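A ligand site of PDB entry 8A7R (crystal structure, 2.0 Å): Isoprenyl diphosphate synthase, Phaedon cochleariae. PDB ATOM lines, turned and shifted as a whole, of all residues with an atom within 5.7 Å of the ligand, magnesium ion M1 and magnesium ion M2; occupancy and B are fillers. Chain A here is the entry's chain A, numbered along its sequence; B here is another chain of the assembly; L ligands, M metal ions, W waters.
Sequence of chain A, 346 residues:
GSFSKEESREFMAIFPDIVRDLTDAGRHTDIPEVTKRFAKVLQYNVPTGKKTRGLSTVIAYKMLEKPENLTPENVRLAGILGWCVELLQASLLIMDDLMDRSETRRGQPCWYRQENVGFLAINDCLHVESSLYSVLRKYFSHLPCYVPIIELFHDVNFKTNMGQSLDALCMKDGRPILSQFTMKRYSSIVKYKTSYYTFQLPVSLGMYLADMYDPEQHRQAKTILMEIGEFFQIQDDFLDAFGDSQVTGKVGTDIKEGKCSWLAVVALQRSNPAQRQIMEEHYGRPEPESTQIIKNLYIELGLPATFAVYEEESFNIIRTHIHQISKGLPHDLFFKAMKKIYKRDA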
ATOM      1  N   SER A  91       7.720 -10.437  -5.353  1.00  0.00           N
ATOM      2  CA  SER A  91       6.646 -11.277  -5.935  1.00  0.00           C
ATOM      3  C   SER A  91       6.008 -10.549  -7.134  1.00  0.00           C
ATOM      4  O   SER A  91       5.815 -11.203  -8.172  1.00  0.00           O
ATOM      5  CB  SER A  91       5.609 -11.659  -4.906  1.00  0.00           C
ATOM      6  OG  SER A  91       4.904 -10.512  -4.453  1.00  0.00           O
ATOM      7  N   LEU A  92       5.701  -9.261  -6.977  1.00  0.00           N
ATOM      8  CA  LEU A  92       5.013  -8.442  -8.021  1.00  0.00           C
ATOM      9  C   LEU A  92       5.894  -8.328  -9.267  1.00  0.00           C
ATOM     10  O   LEU A  92       5.362  -8.462 -10.382  1.00  0.00           O
ATOM     11  CB  LEU A  92       4.699  -7.037  -7.479  1.00  0.00           C
ATOM     12  CG  LEU A  92       3.739  -6.954  -6.294  1.00  0.00           C
ATOM     13  CD1 LEU A  92       3.700  -5.519  -5.762  1.00  0.00           C
ATOM     14  CD2 LEU A  92       2.353  -7.437  -6.665  1.00  0.00           C
ATOM     15  N   LEU A  93       7.195  -8.074  -9.075  1.00  0.00           N
ATOM     16  CA  LEU A  93       8.162  -7.826 -10.175  1.00  0.00           C
ATOM     17  C   LEU A  93       8.501  -9.140 -10.890  1.00  0.00           C
ATOM     18  O   LEU A  93       8.698  -9.086 -12.120  1.00  0.00           O
ATOM     19  CB  LEU A  93       9.408  -7.134  -9.622  1.00  0.00           C
ATOM     20  CG  LEU A  93       9.167  -5.756  -9.000  1.00  0.00           C
ATOM     21  CD1 LEU A  93      10.473  -5.126  -8.536  1.00  0.00           C
ATOM     22  CD2 LEU A  93       8.456  -4.818  -9.979  1.00  0.00           C
ATOM     23  N   MET A  95       6.349 -11.513 -11.370  1.00  0.00           N
ATOM     24  CA  MET A  95       5.130 -11.698 -12.186  1.00  0.00           C
ATOM     25  C   MET A  95       5.099 -10.656 -13.312  1.00  0.00           C
ATOM     26  O   MET A  95       4.791 -11.042 -14.459  1.00  0.00           O
ATOM     27  CB  MET A  95       3.860 -11.536 -11.346  1.00  0.00           C
ATOM     28  CG  MET A  95       2.602 -11.691 -12.187  1.00  0.00           C
ATOM     29  SD  MET A  95       1.188 -12.150 -11.197  1.00  0.00           S
ATOM     30  CE  MET A  95       1.504 -13.893 -10.967  1.00  0.00           C
ATOM     31  N   ASP A  96       5.406  -9.398 -13.002  1.00  0.00           N
ATOM     32  CA  ASP A  96       5.313  -8.288 -13.988  1.00  0.00           C
ATOM     33  C   ASP A  96       6.298  -8.531 -15.130  1.00  0.00           C
ATOM     34  O   ASP A  96       5.934  -8.240 -16.287  1.00  0.00           O
ATOM     35  CB  ASP A  96       5.563  -6.910 -13.374  1.00  0.00           C
ATOM     36  CG  ASP A  96       5.501  -5.820 -14.424  1.00  0.00           C
ATOM     37  OD1 ASP A  96       6.566  -5.250 -14.739  1.00  0.00           O
ATOM     38  OD2 ASP A  96       4.393  -5.596 -14.967  1.00  0.00           O
ATOM     39  N   ASP A  97       7.498  -9.030 -14.816  1.00  0.00           N
ATOM     40  CA  ASP A  97       8.563  -9.311 -15.820  1.00  0.00           C
ATOM     41  C   ASP A  97       8.100 -10.424 -16.764  1.00  0.00           C
ATOM     42  O   ASP A  97       8.348 -10.292 -17.981  1.00  0.00           O
ATOM     43  CB  ASP A  97       9.905  -9.613 -15.142  1.00  0.00           C
ATOM     44  CG  ASP A  97      10.532  -8.384 -14.491  1.00  0.00           C
ATOM     45  OD1 ASP A  97      10.150  -7.264 -14.868  1.00  0.00           O
ATOM     46  OD2 ASP A  97      11.391  -8.572 -13.607  1.00  0.00           O
ATOM     47  N   MET A  99       4.862 -11.073 -17.417  1.00  0.00           N
ATOM     48  CA  MET A  99       3.734 -10.418 -18.141  1.00  0.00           C
ATOM     49  C   MET A  99       4.282  -9.481 -19.233  1.00  0.00           C
ATOM     50  O   MET A  99       3.747  -9.496 -20.343  1.00  0.00           O
ATOM     51  CB  MET A  99       2.843  -9.634 -17.171  1.00  0.00           C
ATOM     52  CG  MET A  99       2.031 -10.551 -16.264  1.00  0.00           C
ATOM     53  SD  MET A  99       1.001  -9.670 -15.066  1.00  0.00           S
ATOM     54  CE  MET A  99      -0.219  -8.952 -16.159  1.00  0.00           C
ATOM     55  N   ASP A 100       5.328  -8.701 -18.931  1.00  0.00           N
ATOM     56  CA  ASP A 100       5.922  -7.712 -19.885  1.00  0.00           C
ATOM     57  C   ASP A 100       6.908  -8.413 -20.829  1.00  0.00           C
ATOM     58  O   ASP A 100       7.308  -7.779 -21.830  1.00  0.00           O
ATOM     59  CB  ASP A 100       6.585  -6.568 -19.130  1.00  0.00           C
ATOM     60  CG  ASP A 100       5.602  -5.607 -18.479  1.00  0.00           C
ATOM     61  OD1 ASP A 100       4.375  -5.806 -18.659  1.00  0.00           O
ATOM     62  OD2 ASP A 100       6.056  -4.679 -17.795  1.00  0.00           O
ATOM     63  N   SER A 102       9.979  -8.938 -20.170  1.00  0.00           N
ATOM     64  CA  SER A 102      11.190  -8.077 -20.034  1.00  0.00           C
ATOM     65  C   SER A 102      12.451  -8.934 -20.063  1.00  0.00           C
ATOM     66  O   SER A 102      12.363 -10.150 -19.771  1.00  0.00           O
ATOM     67  CB  SER A 102      11.118  -7.233 -18.790  1.00  0.00           C
ATOM     68  OG  SER A 102       9.976  -6.394 -18.816  1.00  0.00           O
ATOM     69  N   ARG A 105      15.984  -7.056 -14.988  1.00  0.00           N
ATOM     70  CA  ARG A 105      15.509  -6.242 -13.843  1.00  0.00           C
ATOM     71  C   ARG A 105      16.675  -6.158 -12.843  1.00  0.00           C
ATOM     72  O   ARG A 105      17.298  -7.211 -12.586  1.00  0.00           O
ATOM     73  CB  ARG A 105      14.232  -6.857 -13.264  1.00  0.00           C
ATOM     74  CG  ARG A 105      14.034  -6.636 -11.773  1.00  0.00           C
ATOM     75  CD  ARG A 105      12.776  -5.886 -11.371  1.00  0.00           C
ATOM     76  NE  ARG A 105      11.691  -5.860 -12.346  1.00  0.00           N
ATOM     77  CZ  ARG A 105      10.957  -4.791 -12.662  1.00  0.00           C
ATOM     78  NH1 ARG A 105      11.213  -3.612 -12.111  1.00  0.00           N
ATOM     79  NH2 ARG A 105       9.977  -4.900 -13.539  1.00  0.00           N
ATOM     80  N   ASN A 157      -2.032  -5.878  -1.605  1.00  0.00           N
ATOM     81  CA  ASN A 157      -1.876  -6.900  -2.677  1.00  0.00           C
ATOM     82  C   ASN A 157      -3.086  -6.819  -3.619  1.00  0.00           C
ATOM     83  O   ASN A 157      -2.891  -6.741  -4.846  1.00  0.00           O
ATOM     84  CB  ASN A 157      -1.688  -8.309  -2.113  1.00  0.00           C
ATOM     85  CG  ASN A 157      -1.335  -9.321  -3.177  1.00  0.00           C
ATOM     86  OD1 ASN A 157      -2.188  -9.745  -3.961  1.00  0.00           O
ATOM     87  ND2 ASN A 157      -0.076  -9.725  -3.224  1.00  0.00           N
ATOM     88  N   THR A 160      -3.059  -3.518  -5.625  1.00  0.00           N
ATOM     89  CA  THR A 160      -1.954  -3.518  -6.631  1.00  0.00           C
ATOM     90  C   THR A 160      -2.390  -4.350  -7.840  1.00  0.00           C
ATOM     91  O   THR A 160      -2.084  -3.945  -8.979  1.00  0.00           O
ATOM     92  CB  THR A 160      -0.639  -3.999  -6.014  1.00  0.00           C
ATOM     93  OG1 THR A 160      -0.412  -3.264  -4.808  1.00  0.00           O
ATOM     94  CG2 THR A 160       0.540  -3.804  -6.946  1.00  0.00           C
ATOM     95  N   ASN A 161      -3.127  -5.434  -7.609  1.00  0.00           N
ATOM     96  CA  ASN A 161      -3.676  -6.297  -8.684  1.00  0.00           C
ATOM     97  C   ASN A 161      -4.683  -5.490  -9.518  1.00  0.00           C
ATOM     98  O   ASN A 161      -4.600  -5.567 -10.750  1.00  0.00           O
ATOM     99  CB  ASN A 161      -4.254  -7.603  -8.123  1.00  0.00           C
ATOM    100  CG  ASN A 161      -3.208  -8.690  -8.030  1.00  0.00           C
ATOM    101  OD1 ASN A 161      -2.767  -9.224  -9.045  1.00  0.00           O
ATOM    102  ND2 ASN A 161      -2.791  -9.015  -6.814  1.00  0.00           N
ATOM    103  N   GLN A 164      -2.612  -3.199 -11.734  1.00  0.00           N
ATOM    104  CA  GLN A 164      -2.011  -3.996 -12.848  1.00  0.00           C
ATOM    105  C   GLN A 164      -3.091  -4.257 -13.899  1.00  0.00           C
ATOM    106  O   GLN A 164      -2.815  -4.044 -15.097  1.00  0.00           O
ATOM    107  CB  GLN A 164      -1.411  -5.294 -12.326  1.00  0.00           C
ATOM    108  CG  GLN A 164      -0.681  -6.119 -13.375  1.00  0.00           C
ATOM    109  CD  GLN A 164       0.701  -5.603 -13.701  1.00  0.00           C
ATOM    110  OE1 GLN A 164       0.942  -4.401 -13.729  1.00  0.00           O
ATOM    111  NE2 GLN A 164       1.615  -6.524 -13.960  1.00  0.00           N
ATOM    112  N   ASP A 167      -4.052  -1.100 -15.854  1.00  0.00           N
ATOM    113  CA  ASP A 167      -2.937  -0.891 -16.819  1.00  0.00           C
ATOM    114  C   ASP A 167      -3.207  -1.745 -18.066  1.00  0.00           C
ATOM    115  O   ASP A 167      -3.090  -1.205 -19.185  1.00  0.00           O
ATOM    116  CB  ASP A 167      -1.581  -1.224 -16.182  1.00  0.00           C
ATOM    117  CG  ASP A 167      -0.392  -0.501 -16.795  1.00  0.00           C
ATOM    118  OD1 ASP A 167      -0.596   0.605 -17.328  1.00  0.00           O
ATOM    119  OD2 ASP A 167       0.725  -1.035 -16.712  1.00  0.00           O
ATOM    120  N   LYS A 193      -1.497   0.755  -8.718  1.00  0.00           N
ATOM    121  CA  LYS A 193      -0.426  -0.166  -9.192  1.00  0.00           C
ATOM    122  C   LYS A 193       0.877   0.093  -8.421  1.00  0.00           C
ATOM    123  O   LYS A 193       1.618  -0.888  -8.227  1.00  0.00           O
ATOM    124  CB  LYS A 193      -0.192  -0.054 -10.699  1.00  0.00           C
ATOM    125  CG  LYS A 193       0.617  -1.200 -11.289  1.00  0.00           C
ATOM    126  CD  LYS A 193       0.983  -1.013 -12.743  1.00  0.00           C
ATOM    127  CE  LYS A 193       2.057   0.024 -12.963  1.00  0.00           C
ATOM    128  NZ  LYS A 193       2.569  -0.009 -14.351  1.00  0.00           N
ATOM    129  N   THR A 194       1.175   1.331  -8.021  1.00  0.00           N
ATOM    130  CA  THR A 194       2.512   1.683  -7.456  1.00  0.00           C
ATOM    131  C   THR A 194       2.400   2.373  -6.094  1.00  0.00           C
ATOM    132  O   THR A 194       3.103   1.918  -5.174  1.00  0.00           O
ATOM    133  CB  THR A 194       3.342   2.485  -8.472  1.00  0.00           C
ATOM    134  OG1 THR A 194       2.702   3.731  -8.729  1.00  0.00           O
ATOM    135  CG2 THR A 194       3.544   1.734  -9.773  1.00  0.00           C
ATOM    136  N   TYR A 197       1.641   0.331  -2.512  1.00  0.00           N
ATOM    137  CA  TYR A 197       2.704  -0.596  -2.014  1.00  0.00           C
ATOM    138  C   TYR A 197       4.017   0.178  -1.807  1.00  0.00           C
ATOM    139  O   TYR A 197       4.796  -0.232  -0.935  1.00  0.00           O
ATOM    140  CB  TYR A 197       2.846  -1.821  -2.917  1.00  0.00           C
ATOM    141  CG  TYR A 197       3.927  -1.753  -3.958  1.00  0.00           C
ATOM    142  CD1 TYR A 197       5.222  -2.176  -3.668  1.00  0.00           C
ATOM    143  CD2 TYR A 197       3.674  -1.293  -5.230  1.00  0.00           C
ATOM    144  CE1 TYR A 197       6.225  -2.124  -4.616  1.00  0.00           C
ATOM    145  CE2 TYR A 197       4.667  -1.243  -6.200  1.00  0.00           C
ATOM    146  CZ  TYR A 197       5.947  -1.657  -5.894  1.00  0.00           C
ATOM    147  OH  TYR A 197       6.927  -1.602  -6.835  1.00  0.00           O
ATOM    148  N   ASP A 254       9.307   2.430 -22.612  1.00  0.00           N
ATOM    149  CA  ASP A 254       7.880   2.806 -22.375  1.00  0.00           C
ATOM    150  C   ASP A 254       7.165   2.977 -23.722  1.00  0.00           C
ATOM    151  O   ASP A 254       6.023   2.474 -23.849  1.00  0.00           O
ATOM    152  CB  ASP A 254       7.754   4.082 -21.549  1.00  0.00           C
ATOM    153  CG  ASP A 254       7.996   3.889 -20.057  1.00  0.00           C
ATOM    154  OD1 ASP A 254       7.772   4.862 -19.304  1.00  0.00           O
ATOM    155  OD2 ASP A 254       8.394   2.784 -19.661  1.00  0.00           O
ATOM    156  N   GLU A 257       6.888  -0.423 -25.586  1.00  0.00           N
ATOM    157  CA  GLU A 257       5.937  -1.300 -24.854  1.00  0.00           C
ATOM    158  C   GLU A 257       4.515  -0.709 -24.906  1.00  0.00           C
ATOM    159  O   GLU A 257       3.577  -1.417 -24.501  1.00  0.00           O
ATOM    160  CB  GLU A 257       6.401  -1.517 -23.414  1.00  0.00           C
ATOM    161  CG  GLU A 257       7.650  -2.384 -23.326  1.00  0.00           C
ATOM    162  CD  GLU A 257       8.053  -2.797 -21.915  1.00  0.00           C
ATOM    163  OE1 GLU A 257       7.154  -3.097 -21.108  1.00  0.00           O
ATOM    164  OE2 GLU A 257       9.269  -2.815 -21.636  1.00  0.00           O
ATOM    165  N   LYS A 259       3.199   1.855 -23.188  1.00  0.00           N
ATOM    166  CA  LYS A 259       2.723   2.041 -21.791  1.00  0.00           C
ATOM    167  C   LYS A 259       1.884   3.315 -21.699  1.00  0.00           C
ATOM    168  O   LYS A 259       2.177   4.279 -22.437  1.00  0.00           O
ATOM    169  CB  LYS A 259       3.906   2.133 -20.823  1.00  0.00           C
ATOM    170  CG  LYS A 259       4.775   0.902 -20.777  1.00  0.00           C
ATOM    171  CD  LYS A 259       5.183   0.498 -19.379  1.00  0.00           C
ATOM    172  CE  LYS A 259       6.002  -0.769 -19.360  1.00  0.00           C
ATOM    173  NZ  LYS A 259       6.685  -0.945 -18.046  1.00  0.00           N
ATOM    174  N   ASN B 123      -1.983 -12.203 -13.730  1.00  0.00           N
ATOM    175  CA  ASN B 123      -2.110 -11.728 -12.323  1.00  0.00           C
ATOM    176  C   ASN B 123      -3.492 -12.042 -11.745  1.00  0.00           C
ATOM    177  O   ASN B 123      -3.691 -11.801 -10.546  1.00  0.00           O
ATOM    178  CB  ASN B 123      -1.797 -10.228 -12.195  1.00  0.00           C
ATOM    179  CG  ASN B 123      -2.846  -9.341 -12.816  1.00  0.00           C
ATOM    180  OD1 ASN B 123      -3.033  -9.346 -14.028  1.00  0.00           O
ATOM    181  ND2 ASN B 123      -3.547  -8.572 -11.989  1.00  0.00           N
ATOM    182  N   LEU B 126      -3.195 -14.536  -8.788  1.00  0.00           N
ATOM    183  CA  LEU B 126      -2.749 -13.813  -7.564  1.00  0.00           C
ATOM    184  C   LEU B 126      -3.941 -13.044  -6.982  1.00  0.00           C
ATOM    185  O   LEU B 126      -4.160 -13.120  -5.748  1.00  0.00           O
ATOM    186  CB  LEU B 126      -1.604 -12.865  -7.927  1.00  0.00           C
ATOM    187  CG  LEU B 126      -1.058 -11.993  -6.792  1.00  0.00           C
ATOM    188  CD1 LEU B 126      -0.495 -12.846  -5.667  1.00  0.00           C
ATOM    189  CD2 LEU B 126      -0.004 -11.034  -7.317  1.00  0.00           C
HETATM  190  C1  LIG L   1       5.664  -2.713 -12.586  1.00  0.00           C
HETATM  191  O1  LIG L   1       4.963  -1.928 -13.547  1.00  0.00           O
HETATM  192  C2  LIG L   1       4.680  -3.542 -11.810  1.00  0.00           C
HETATM  193  C3  LIG L   1       4.356  -3.401 -10.519  1.00  0.00           C
HETATM  194  C4  LIG L   1       5.088  -2.512  -9.559  1.00  0.00           C
HETATM  195  C5  LIG L   1       3.183  -4.134  -9.922  1.00  0.00           C
HETATM  196  C6  LIG L   1       2.655  -5.286 -10.755  1.00  0.00           C
HETATM  197  C7  LIG L   1       1.444  -5.921 -10.161  1.00  0.00           C
HETATM  198  C8  LIG L   1       1.008  -7.171 -10.277  1.00  0.00           C
HETATM  199  C9  LIG L   1       1.818  -8.277 -10.890  1.00  0.00           C
HETATM  200  C10 LIG L   1      -0.354  -7.581  -9.825  1.00  0.00           C
HETATM  201  P1  LIG L   1       5.700  -1.465 -14.899  1.00  0.00           P
HETATM  202  O2  LIG L   1       5.881  -2.654 -15.788  1.00  0.00           O
HETATM  203  O3  LIG L   1       4.979  -0.284 -15.439  1.00  0.00           O
HETATM  204  O4  LIG L   1       7.130  -0.986 -14.342  1.00  0.00           O
HETATM  205  P2  LIG L   1       8.632  -1.569 -14.442  1.00  0.00           P
HETATM  206  O5  LIG L   1       8.551  -2.968 -14.999  1.00  0.00           O
HETATM  207  O6  LIG L   1       9.165  -1.547 -13.028  1.00  0.00           O
HETATM  208  O7  LIG L   1       9.362  -0.625 -15.357  1.00  0.00           O
HETATM  209 MG    MG M   1       3.810  -4.179 -16.770  1.00  0.00          MG
HETATM  210 MG    MG M   2       7.330  -4.050 -16.311  1.00  0.00          MG
HETATM  211 MG    MG M   3       9.516   3.238 -15.564  1.00  0.00          MG
HETATM  212  O   HOH W   1       1.971  -5.454 -17.310  1.00  0.00           O
HETATM  213  O   HOH W   2       8.736  -5.496 -16.623  1.00  0.00           O
HETATM  214  O   HOH W   3       7.921   2.445 -14.837  1.00  0.00           O
HETATM  215  O   HOH W   4       8.247  -3.075 -17.964  1.00  0.00           O
HETATM  216  O   HOH W   5       3.478  -3.099 -18.206  1.00  0.00           O
HETATM  217  O   HOH W   6       2.360  -2.973 -15.617  1.00  0.00           O
HETATM  218  O   HOH W   7      10.429   1.672 -15.270  1.00  0.00           O
HETATM  219  O   HOH W   8       8.868   2.086 -17.339  1.00  0.00           O
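NZ of Lys 193 lies within salt-bridge range of O3 of the ligand, at 2.7 Å. The guanidinium group (NH1) of Arg 105 is in salt-bridge range of an oxygen (O6) of the ligand. NZ of Lys 259 is in salt-bridge range of O3 of the ligand, 3.2 Å away.
The side-chain amino group (NZ) of Lys 259 lies close to the side-chain carboxylate (OD2) of Asp 100 (3.8 Å). NH2 of Arg 105 sits close to OD1 of Asp 96, 3.6 Å away. The side-chain carboxylate (OD2) of Asp 167 lies within salt-bridge range of the side-chain amino group (NZ) of Lys 193 (3.2 Å). The side-chain carboxylate of Asp 97 lies within salt-bridge range of the guanidinium group of Arg 105. The side-chain amino group (NZ) of Lys 259 is in salt-bridge range of the side-chain carboxylate (OE1) of Glu 257 (3.8 Å). The backbone carbonyl oxygen of Asp 254 is in hydrogen-bond range of the backbone NH of Lys 259. The side-chain amide nitrogen of Asn 123 of chain B is in hydrogen-bond range of the side-chain amide oxygen of Asn 161, 3.1 Å away. NE2 of Gln 164 lies within hydrogen-bond range of SD of Met 99, at 3.4 Å.
Merely in contact with the ligand: Asn 161, Tyr 197, Gln 164, Leu 92, Met 95, Asn 123 of chain B and Thr 160. Hydrophobic or aromatic side chains that line the ligand: Leu 92, Met 95 and Tyr 197. Of the 23 residues printed, 12 come within 4 Å of the ligand.
Within 4 Å of magnesium ion M1: Asp 96 and Asp 100.
Residues that only touch magnesium ion M2: Lys 259 (3.6 Å) and Arg 105 (3.9 Å). The nearest printed residue that does not touch magnesium ion M2 is Ser 102 (4.3 Å).
Magnesium ion M1 is bound by water W5 (1.8 Å). Water W6 binds magnesium ion M1, 2.2 Å away. Water W1 is bound to magnesium ion M1 (2.3 Å). Magnesium ion M1 is bound by the side-chain carboxylate (OD2) of Asp 96 (2.4 Å). OD2 of Asp 100 binds magnesium ion M1, at 2.5 Å. Magnesium ion M1 is bound by OD1 of Asp 100. Magnesium ion M1 has six donor atoms within binding distance. Slightly farther from magnesium ion M1 lies an oxygen (O2) of the ligand (2.8 Å).
Magnesium ion M2 is bound by water W2, 2.0 Å away. OD2 of Asp 100 is bound to magnesium ion M2 (2.1 Å). O2 of the ligand binds magnesium ion M2. Magnesium ion M2 is bound by O5 of the ligand, at 2.1 Å. OD1 of Asp 96 binds magnesium ion M2 (2.1 Å). Water W4 binds magnesium ion M2, 2.1 Å away. Magnesium ion M2 has six donor atoms within binding distance.
Water W4 lies within hydrogen-bond range of NZ of Lys 259 (2.6 Å) and OE1 of Glu 257 (3.3 Å). Water W2 lies within hydrogen-bond range of OG of Ser 102 (2.7 Å), OD1 of Asp 97 (2.9 Å) and NH2 of Arg 105 (3.4 Å). Water W8 lies within hydrogen-bond range of the side-chain carboxylate of Asp 254 (2.5 Å) and an oxygen (O7) of the ligand (3.4 Å).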
